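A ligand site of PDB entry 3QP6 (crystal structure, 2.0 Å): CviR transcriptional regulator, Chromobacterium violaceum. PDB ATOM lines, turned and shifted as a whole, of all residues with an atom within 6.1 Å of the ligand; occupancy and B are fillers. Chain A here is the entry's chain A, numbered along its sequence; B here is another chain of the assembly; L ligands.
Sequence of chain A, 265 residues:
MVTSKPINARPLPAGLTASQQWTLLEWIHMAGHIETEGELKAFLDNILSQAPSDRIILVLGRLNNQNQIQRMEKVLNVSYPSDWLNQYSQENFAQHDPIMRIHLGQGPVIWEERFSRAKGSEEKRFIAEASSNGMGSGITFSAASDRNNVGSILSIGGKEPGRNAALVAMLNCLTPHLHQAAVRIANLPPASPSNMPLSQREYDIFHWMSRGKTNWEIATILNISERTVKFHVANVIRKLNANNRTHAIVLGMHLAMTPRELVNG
The indole nitrogen (NE1) of Trp 111 is in hydrogen-bond range of the side-chain hydroxyl (OG1) of Thr 140 (2.9 Å).
The backbone carbonyl oxygen (O) of Ile 57 lies within hydrogen-bond range of the backbone NH (N) of Ser 155 (2.9 Å).
The backbone carbonyl oxygen of Ala 130 sits at hydrogen-bond distance from the backbone NH of Met 135, at 2.8 Å.
The backbone NH of Ile 153 sits at hydrogen-bond distance from the backbone carbonyl oxygen of Val 59 (2.9 Å).
OH of Tyr 88 lies within hydrogen-bond range of OD2 of Asp 97, at 2.6 Å.
The side-chain hydroxyl (OG) of Ser 155 lies within hydrogen-bond range of the side-chain hydroxyl (OG1) of Thr 140 (2.7 Å).
N of Ile 99 lies within hydrogen-bond range of OD1 of Asp 97.
Residues that only touch the ligand: Met 135, Ile 153, Phe 126, Ile 99, Trp 111, Phe 115, Leu 85, Tyr 88, Val 59, Ala 130 and Met 257 of chain B.
Hydrophobic or aromatic side chains that line the ligand: Val 59, Tyr 80, Trp 84, Leu 85, Tyr 88, Ile 99, Trp 111, Phe 115, Phe 126, Ala 130, Met 135, Ile 153 and Met 257 of chain B.
Within 4 Å of the ligand: Val 59, Tyr 80, Trp 84, Leu 85, Tyr 88, Asp 97, Ile 99, Trp 111, Phe 115, Phe 126, Ala 130, Met 135, Ile 153, Ser 155 and Met 257 of chain B.
A nitrogen (N1) of the ligand is in hydrogen-bond range of the side-chain carboxylate of Asp 97, 2.7 Å away.
An oxygen (O3) of the ligand sits at hydrogen-bond distance from the side-chain hydroxyl (OG) of Ser 155.
OH of Tyr 80 sits at hydrogen-bond distance from O3 of the ligand.
NE1 of Trp 84 lies within hydrogen-bond range of O1 of the ligand (3.0 Å).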
ATOM      1  N   ILE A  57     -12.389  12.280 -20.963  1.00  0.00           N
ATOM      2  CA  ILE A  57     -13.174  12.799 -19.859  1.00  0.00           C
ATOM      3  C   ILE A  57     -14.653  12.812 -20.247  1.00  0.00           C
ATOM      4  O   ILE A  57     -15.002  12.904 -21.429  1.00  0.00           O
ATOM      5  CB  ILE A  57     -12.701  14.208 -19.440  1.00  0.00           C
ATOM      6  CG1 ILE A  57     -13.203  14.582 -18.037  1.00  0.00           C
ATOM      7  CG2 ILE A  57     -13.143  15.255 -20.474  1.00  0.00           C
ATOM      8  CD1 ILE A  57     -12.333  15.652 -17.357  1.00  0.00           C
ATOM      9  N   VAL A  59     -18.121  14.939 -18.991  1.00  0.00           N
ATOM     10  CA  VAL A  59     -18.643  16.044 -18.184  1.00  0.00           C
ATOM     11  C   VAL A  59     -20.166  16.103 -18.306  1.00  0.00           C
ATOM     12  O   VAL A  59     -20.720  16.170 -19.416  1.00  0.00           O
ATOM     13  CB  VAL A  59     -18.033  17.391 -18.576  1.00  0.00           C
ATOM     14  CG1 VAL A  59     -18.753  18.550 -17.846  1.00  0.00           C
ATOM     15  CG2 VAL A  59     -16.546  17.422 -18.265  1.00  0.00           C
ATOM     16  N   MET A  72     -21.628  22.803 -14.608  1.00  0.00           N
ATOM     17  CA  MET A  72     -21.319  21.385 -14.534  1.00  0.00           C
ATOM     18  C   MET A  72     -22.020  20.764 -13.334  1.00  0.00           C
ATOM     19  O   MET A  72     -22.165  21.408 -12.287  1.00  0.00           O
ATOM     20  CB  MET A  72     -19.801  21.185 -14.442  1.00  0.00           C
ATOM     21  CG  MET A  72     -19.059  21.600 -15.716  1.00  0.00           C
ATOM     22  SD  MET A  72     -17.283  21.340 -15.538  1.00  0.00           S
ATOM     23  CE  MET A  72     -16.649  22.183 -16.981  1.00  0.00           C
ATOM     24  N   VAL A  75     -17.937  15.986 -12.987  1.00  0.00           N
ATOM     25  CA  VAL A  75     -16.763  15.771 -13.806  1.00  0.00           C
ATOM     26  C   VAL A  75     -16.259  14.355 -13.570  1.00  0.00           C
ATOM     27  O   VAL A  75     -15.849  13.987 -12.458  1.00  0.00           O
ATOM     28  CB  VAL A  75     -15.667  16.817 -13.505  1.00  0.00           C
ATOM     29  CG1 VAL A  75     -14.380  16.473 -14.231  1.00  0.00           C
ATOM     30  CG2 VAL A  75     -16.158  18.206 -13.905  1.00  0.00           C
ATOM     31  N   TYR A  80      -7.685  12.620 -18.399  1.00  0.00           N
ATOM     32  CA  TYR A  80      -7.147  13.979 -18.522  1.00  0.00           C
ATOM     33  C   TYR A  80      -6.026  14.161 -17.498  1.00  0.00           C
ATOM     34  O   TYR A  80      -6.149  13.688 -16.374  1.00  0.00           O
ATOM     35  CB  TYR A  80      -8.256  15.026 -18.330  1.00  0.00           C
ATOM     36  CG  TYR A  80      -8.948  15.451 -19.620  1.00  0.00           C
ATOM     37  CD1 TYR A  80      -9.117  14.551 -20.667  1.00  0.00           C
ATOM     38  CD2 TYR A  80      -9.439  16.738 -19.779  1.00  0.00           C
ATOM     39  CE1 TYR A  80      -9.761  14.937 -21.856  1.00  0.00           C
ATOM     40  CE2 TYR A  80     -10.087  17.136 -20.951  1.00  0.00           C
ATOM     41  CZ  TYR A  80     -10.247  16.228 -21.991  1.00  0.00           C
ATOM     42  OH  TYR A  80     -10.864  16.615 -23.160  1.00  0.00           O
ATOM     43  N   TRP A  84      -3.520  19.652 -15.992  1.00  0.00           N
ATOM     44  CA  TRP A  84      -4.415  20.374 -16.894  1.00  0.00           C
ATOM     45  C   TRP A  84      -5.776  20.682 -16.238  1.00  0.00           C
ATOM     46  O   TRP A  84      -6.277  21.804 -16.338  1.00  0.00           O
ATOM     47  CB  TRP A  84      -4.571  19.608 -18.225  1.00  0.00           C
ATOM     48  CG  TRP A  84      -5.586  20.207 -19.164  1.00  0.00           C
ATOM     49  CD1 TRP A  84      -6.751  19.625 -19.599  1.00  0.00           C
ATOM     50  CD2 TRP A  84      -5.547  21.511 -19.770  1.00  0.00           C
ATOM     51  NE1 TRP A  84      -7.431  20.487 -20.438  1.00  0.00           N
ATOM     52  CE2 TRP A  84      -6.716  21.653 -20.544  1.00  0.00           C
ATOM     53  CE3 TRP A  84      -4.635  22.577 -19.706  1.00  0.00           C
ATOM     54  CZ2 TRP A  84      -6.981  22.815 -21.285  1.00  0.00           C
ATOM     55  CZ3 TRP A  84      -4.912  23.735 -20.435  1.00  0.00           C
ATOM     56  CH2 TRP A  84      -6.077  23.841 -21.208  1.00  0.00           C
ATOM     57  N   LEU A  85      -6.358  19.708 -15.545  1.00  0.00           N
ATOM     58  CA  LEU A  85      -7.616  19.927 -14.826  1.00  0.00           C
ATOM     59  C   LEU A  85      -7.455  21.020 -13.762  1.00  0.00           C
ATOM     60  O   LEU A  85      -8.312  21.884 -13.576  1.00  0.00           O
ATOM     61  CB  LEU A  85      -8.130  18.628 -14.205  1.00  0.00           C
ATOM     62  CG  LEU A  85      -8.549  17.480 -15.167  1.00  0.00           C
ATOM     63  CD1 LEU A  85      -8.997  16.237 -14.393  1.00  0.00           C
ATOM     64  CD2 LEU A  85      -9.651  17.917 -16.132  1.00  0.00           C
ATOM     65  N   TYR A  88      -7.343  24.267 -15.566  1.00  0.00           N
ATOM     66  CA  TYR A  88      -8.663  24.519 -16.157  1.00  0.00           C
ATOM     67  C   TYR A  88      -9.618  25.068 -15.095  1.00  0.00           C
ATOM     68  O   TYR A  88     -10.371  26.027 -15.326  1.00  0.00           O
ATOM     69  CB  TYR A  88      -9.198  23.206 -16.755  1.00  0.00           C
ATOM     70  CG  TYR A  88     -10.336  23.334 -17.746  1.00  0.00           C
ATOM     71  CD1 TYR A  88     -10.137  23.106 -19.107  1.00  0.00           C
ATOM     72  CD2 TYR A  88     -11.617  23.669 -17.320  1.00  0.00           C
ATOM     73  CE1 TYR A  88     -11.194  23.213 -20.023  1.00  0.00           C
ATOM     74  CE2 TYR A  88     -12.666  23.775 -18.221  1.00  0.00           C
ATOM     75  CZ  TYR A  88     -12.448  23.541 -19.573  1.00  0.00           C
ATOM     76  OH  TYR A  88     -13.489  23.653 -20.464  1.00  0.00           O
ATOM     77  N   ASP A  97     -13.295  28.034 -23.093  1.00  0.00           N
ATOM     78  CA  ASP A  97     -13.097  26.832 -23.912  1.00  0.00           C
ATOM     79  C   ASP A  97     -14.180  26.754 -24.995  1.00  0.00           C
ATOM     80  O   ASP A  97     -15.346  26.523 -24.677  1.00  0.00           O
ATOM     81  CB  ASP A  97     -13.194  25.606 -22.992  1.00  0.00           C
ATOM     82  CG  ASP A  97     -12.921  24.310 -23.702  1.00  0.00           C
ATOM     83  OD1 ASP A  97     -12.804  24.294 -24.944  1.00  0.00           O
ATOM     84  OD2 ASP A  97     -12.811  23.281 -22.993  1.00  0.00           O
ATOM     85  N   ILE A  99     -14.968  24.433 -26.888  1.00  0.00           N
ATOM     86  CA  ILE A  99     -15.682  23.141 -26.808  1.00  0.00           C
ATOM     87  C   ILE A  99     -16.857  23.224 -25.827  1.00  0.00           C
ATOM     88  O   ILE A  99     -17.852  22.518 -25.983  1.00  0.00           O
ATOM     89  CB  ILE A  99     -14.738  21.958 -26.448  1.00  0.00           C
ATOM     90  CG1 ILE A  99     -13.495  22.008 -27.340  1.00  0.00           C
ATOM     91  CG2 ILE A  99     -15.450  20.609 -26.614  1.00  0.00           C
ATOM     92  CD1 ILE A  99     -13.830  22.259 -28.823  1.00  0.00           C
ATOM     93  N   MET A 100     -16.735  24.081 -24.825  1.00  0.00           N
ATOM     94  CA  MET A 100     -17.794  24.261 -23.827  1.00  0.00           C
ATOM     95  C   MET A 100     -19.005  25.034 -24.381  1.00  0.00           C
ATOM     96  O   MET A 100     -20.043  25.084 -23.735  1.00  0.00           O
ATOM     97  CB  MET A 100     -17.266  24.941 -22.558  1.00  0.00           C
ATOM     98  CG  MET A 100     -16.432  24.030 -21.632  1.00  0.00           C
ATOM     99  SD  MET A 100     -17.346  22.563 -21.058  1.00  0.00           S
ATOM    100  CE  MET A 100     -18.506  23.330 -19.938  1.00  0.00           C
ATOM    101  N   TRP A 111     -12.070  19.273 -32.438  1.00  0.00           N
ATOM    102  CA  TRP A 111     -11.799  20.561 -31.784  1.00  0.00           C
ATOM    103  C   TRP A 111     -11.322  21.666 -32.729  1.00  0.00           C
ATOM    104  O   TRP A 111     -11.702  22.824 -32.561  1.00  0.00           O
ATOM    105  CB  TRP A 111     -10.803  20.422 -30.628  1.00  0.00           C
ATOM    106  CG  TRP A 111     -11.283  19.492 -29.567  1.00  0.00           C
ATOM    107  CD1 TRP A 111     -12.566  19.005 -29.430  1.00  0.00           C
ATOM    108  CD2 TRP A 111     -10.520  18.932 -28.513  1.00  0.00           C
ATOM    109  NE1 TRP A 111     -12.623  18.162 -28.336  1.00  0.00           N
ATOM    110  CE2 TRP A 111     -11.390  18.109 -27.753  1.00  0.00           C
ATOM    111  CE3 TRP A 111      -9.181  19.041 -28.121  1.00  0.00           C
ATOM    112  CZ2 TRP A 111     -10.953  17.397 -26.650  1.00  0.00           C
ATOM    113  CZ3 TRP A 111      -8.756  18.325 -27.006  1.00  0.00           C
ATOM    114  CH2 TRP A 111      -9.642  17.522 -26.288  1.00  0.00           C
ATOM    115  N   PHE A 115     -11.493  25.636 -32.848  1.00  0.00           N
ATOM    116  CA  PHE A 115     -10.267  26.391 -32.587  1.00  0.00           C
ATOM    117  C   PHE A 115      -9.856  27.270 -33.794  1.00  0.00           C
ATOM    118  O   PHE A 115      -9.394  28.391 -33.605  1.00  0.00           O
ATOM    119  CB  PHE A 115      -9.101  25.470 -32.181  1.00  0.00           C
ATOM    120  CG  PHE A 115      -9.310  24.717 -30.881  1.00  0.00           C
ATOM    121  CD1 PHE A 115      -8.379  23.768 -30.459  1.00  0.00           C
ATOM    122  CD2 PHE A 115     -10.422  24.954 -30.083  1.00  0.00           C
ATOM    123  CE1 PHE A 115      -8.555  23.071 -29.273  1.00  0.00           C
ATOM    124  CE2 PHE A 115     -10.602  24.275 -28.887  1.00  0.00           C
ATOM    125  CZ  PHE A 115      -9.666  23.316 -28.481  1.00  0.00           C
ATOM    126  N   PHE A 126      -6.731  30.356 -24.291  1.00  0.00           N
ATOM    127  CA  PHE A 126      -7.099  28.996 -23.923  1.00  0.00           C
ATOM    128  C   PHE A 126      -6.515  28.001 -24.924  1.00  0.00           C
ATOM    129  O   PHE A 126      -5.939  26.975 -24.522  1.00  0.00           O
ATOM    130  CB  PHE A 126      -8.606  28.792 -23.827  1.00  0.00           C
ATOM    131  CG  PHE A 126      -9.001  27.334 -23.747  1.00  0.00           C
ATOM    132  CD1 PHE A 126      -9.298  26.614 -24.901  1.00  0.00           C
ATOM    133  CD2 PHE A 126      -9.015  26.678 -22.520  1.00  0.00           C
ATOM    134  CE1 PHE A 126      -9.631  25.257 -24.834  1.00  0.00           C
ATOM    135  CE2 PHE A 126      -9.338  25.314 -22.446  1.00  0.00           C
ATOM    136  CZ  PHE A 126      -9.647  24.614 -23.604  1.00  0.00           C
ATOM    137  N   ALA A 130      -4.053  25.045 -23.835  1.00  0.00           N
ATOM    138  CA  ALA A 130      -4.401  23.674 -24.182  1.00  0.00           C
ATOM    139  C   ALA A 130      -3.290  23.020 -25.008  1.00  0.00           C
ATOM    140  O   ALA A 130      -2.846  21.905 -24.719  1.00  0.00           O
ATOM    141  CB  ALA A 130      -5.719  23.607 -24.942  1.00  0.00           C
ATOM    142  N   MET A 135      -3.108  19.137 -25.242  1.00  0.00           N
ATOM    143  CA  MET A 135      -4.560  19.066 -25.380  1.00  0.00           C
ATOM    144  C   MET A 135      -5.042  19.828 -26.604  1.00  0.00           C
ATOM    145  O   MET A 135      -6.203  20.282 -26.646  1.00  0.00           O
ATOM    146  CB  MET A 135      -5.243  19.601 -24.111  1.00  0.00           C
ATOM    147  CG  MET A 135      -4.905  18.841 -22.829  1.00  0.00           C
ATOM    148  SD  MET A 135      -5.391  17.084 -22.869  1.00  0.00           S
ATOM    149  CE  MET A 135      -7.141  17.204 -23.255  1.00  0.00           C
ATOM    150  N   GLY A 136      -4.171  19.981 -27.606  1.00  0.00           N
ATOM    151  CA  GLY A 136      -4.474  20.824 -28.748  1.00  0.00           C
ATOM    152  C   GLY A 136      -5.411  20.209 -29.790  1.00  0.00           C
ATOM    153  O   GLY A 136      -6.017  20.923 -30.583  1.00  0.00           O
ATOM    154  N   THR A 140     -15.141  15.726 -29.550  1.00  0.00           N
ATOM    155  CA  THR A 140     -16.128  15.673 -28.487  1.00  0.00           C
ATOM    156  C   THR A 140     -17.472  15.164 -29.007  1.00  0.00           C
ATOM    157  O   THR A 140     -18.021  15.687 -29.977  1.00  0.00           O
ATOM    158  CB  THR A 140     -16.320  17.060 -27.840  1.00  0.00           C
ATOM    159  OG1 THR A 140     -15.132  17.405 -27.130  1.00  0.00           O
ATOM    160  CG2 THR A 140     -17.491  17.059 -26.875  1.00  0.00           C
ATOM    161  N   ILE A 153     -20.950  15.791 -22.300  1.00  0.00           N
ATOM    162  CA  ILE A 153     -19.966  15.704 -23.356  1.00  0.00           C
ATOM    163  C   ILE A 153     -18.959  14.624 -23.023  1.00  0.00           C
ATOM    164  O   ILE A 153     -18.584  14.446 -21.862  1.00  0.00           O
ATOM    165  CB  ILE A 153     -19.236  17.029 -23.602  1.00  0.00           C
ATOM    166  CG1 ILE A 153     -18.547  17.495 -22.331  1.00  0.00           C
ATOM    167  CG2 ILE A 153     -20.200  18.079 -24.088  1.00  0.00           C
ATOM    168  CD1 ILE A 153     -17.249  18.189 -22.591  1.00  0.00           C
ATOM    169  N   SER A 155     -15.270  13.731 -24.206  1.00  0.00           N
ATOM    170  CA  SER A 155     -14.126  14.254 -24.950  1.00  0.00           C
ATOM    171  C   SER A 155     -12.986  13.264 -25.023  1.00  0.00           C
ATOM    172  O   SER A 155     -12.656  12.593 -24.037  1.00  0.00           O
ATOM    173  CB  SER A 155     -13.635  15.573 -24.342  1.00  0.00           C
ATOM    174  OG  SER A 155     -14.546  16.630 -24.621  1.00  0.00           O
ATOM    175  N   ILE A 156     -12.393  13.143 -26.212  1.00  0.00           N
ATOM    176  CA  ILE A 156     -11.192  12.369 -26.377  1.00  0.00           C
ATOM    177  C   ILE A 156     -10.115  13.241 -27.014  1.00  0.00           C
ATOM    178  O   ILE A 156     -10.189  13.576 -28.198  1.00  0.00           O
ATOM    179  CB  ILE A 156     -11.437  11.111 -27.255  1.00  0.00           C
ATOM    180  CG1 ILE A 156     -12.660  10.347 -26.742  1.00  0.00           C
ATOM    181  CG2 ILE A 156     -10.186  10.234 -27.287  1.00  0.00           C
ATOM    182  CD1 ILE A 156     -13.111   9.238 -27.665  1.00  0.00           C
ATOM    183  N   MET B 257     -15.011  24.289 -11.179  1.00  0.00           N
ATOM    184  CA  MET B 257     -14.901  24.647 -12.600  1.00  0.00           C
ATOM    185  C   MET B 257     -15.946  25.635 -13.104  1.00  0.00           C
ATOM    186  O   MET B 257     -15.633  26.463 -13.957  1.00  0.00           O
ATOM    187  CB  MET B 257     -14.903  23.407 -13.472  1.00  0.00           C
ATOM    188  CG  MET B 257     -13.565  22.741 -13.462  1.00  0.00           C
ATOM    189  SD  MET B 257     -13.518  21.275 -14.491  1.00  0.00           S
ATOM    190  CE  MET B 257     -11.740  21.033 -14.448  1.00  0.00           C
HETATM  191  N1  LIG L   1     -12.273  20.761 -23.698  1.00  0.00           N
HETATM  192  C1  LIG L   1      -9.848  20.609 -23.280  1.00  0.00           C
HETATM  193  O1  LIG L   1      -9.903  20.311 -22.094  1.00  0.00           O
HETATM  194  C2  LIG L   1      -8.994  21.497 -25.285  1.00  0.00           C
HETATM  195  O2  LIG L   1      -8.697  21.214 -23.902  1.00  0.00           O
HETATM  196  C3  LIG L   1     -10.530  21.398 -25.391  1.00  0.00           C
HETATM  197  O3  LIG L   1     -12.839  18.569 -23.542  1.00  0.00           O
HETATM  198  C4  LIG L   1     -10.970  20.455 -24.261  1.00  0.00           C
HETATM  199  C5  LIG L   1     -13.085  19.760 -23.347  1.00  0.00           C
HETATM  200  C6  LIG L   1     -14.396  20.166 -22.706  1.00  0.00           C
HETATM  201  C7  LIG L   1     -14.481  19.560 -21.297  1.00  0.00           C
HETATM  202  C8  LIG L   1     -13.211  19.826 -20.474  1.00  0.00           C
HETATM  203  C9  LIG L   1     -13.445  19.601 -18.979  1.00  0.00           C
HETATM  204  C10 LIG L   1     -12.176  19.819 -18.173  1.00  0.00           C
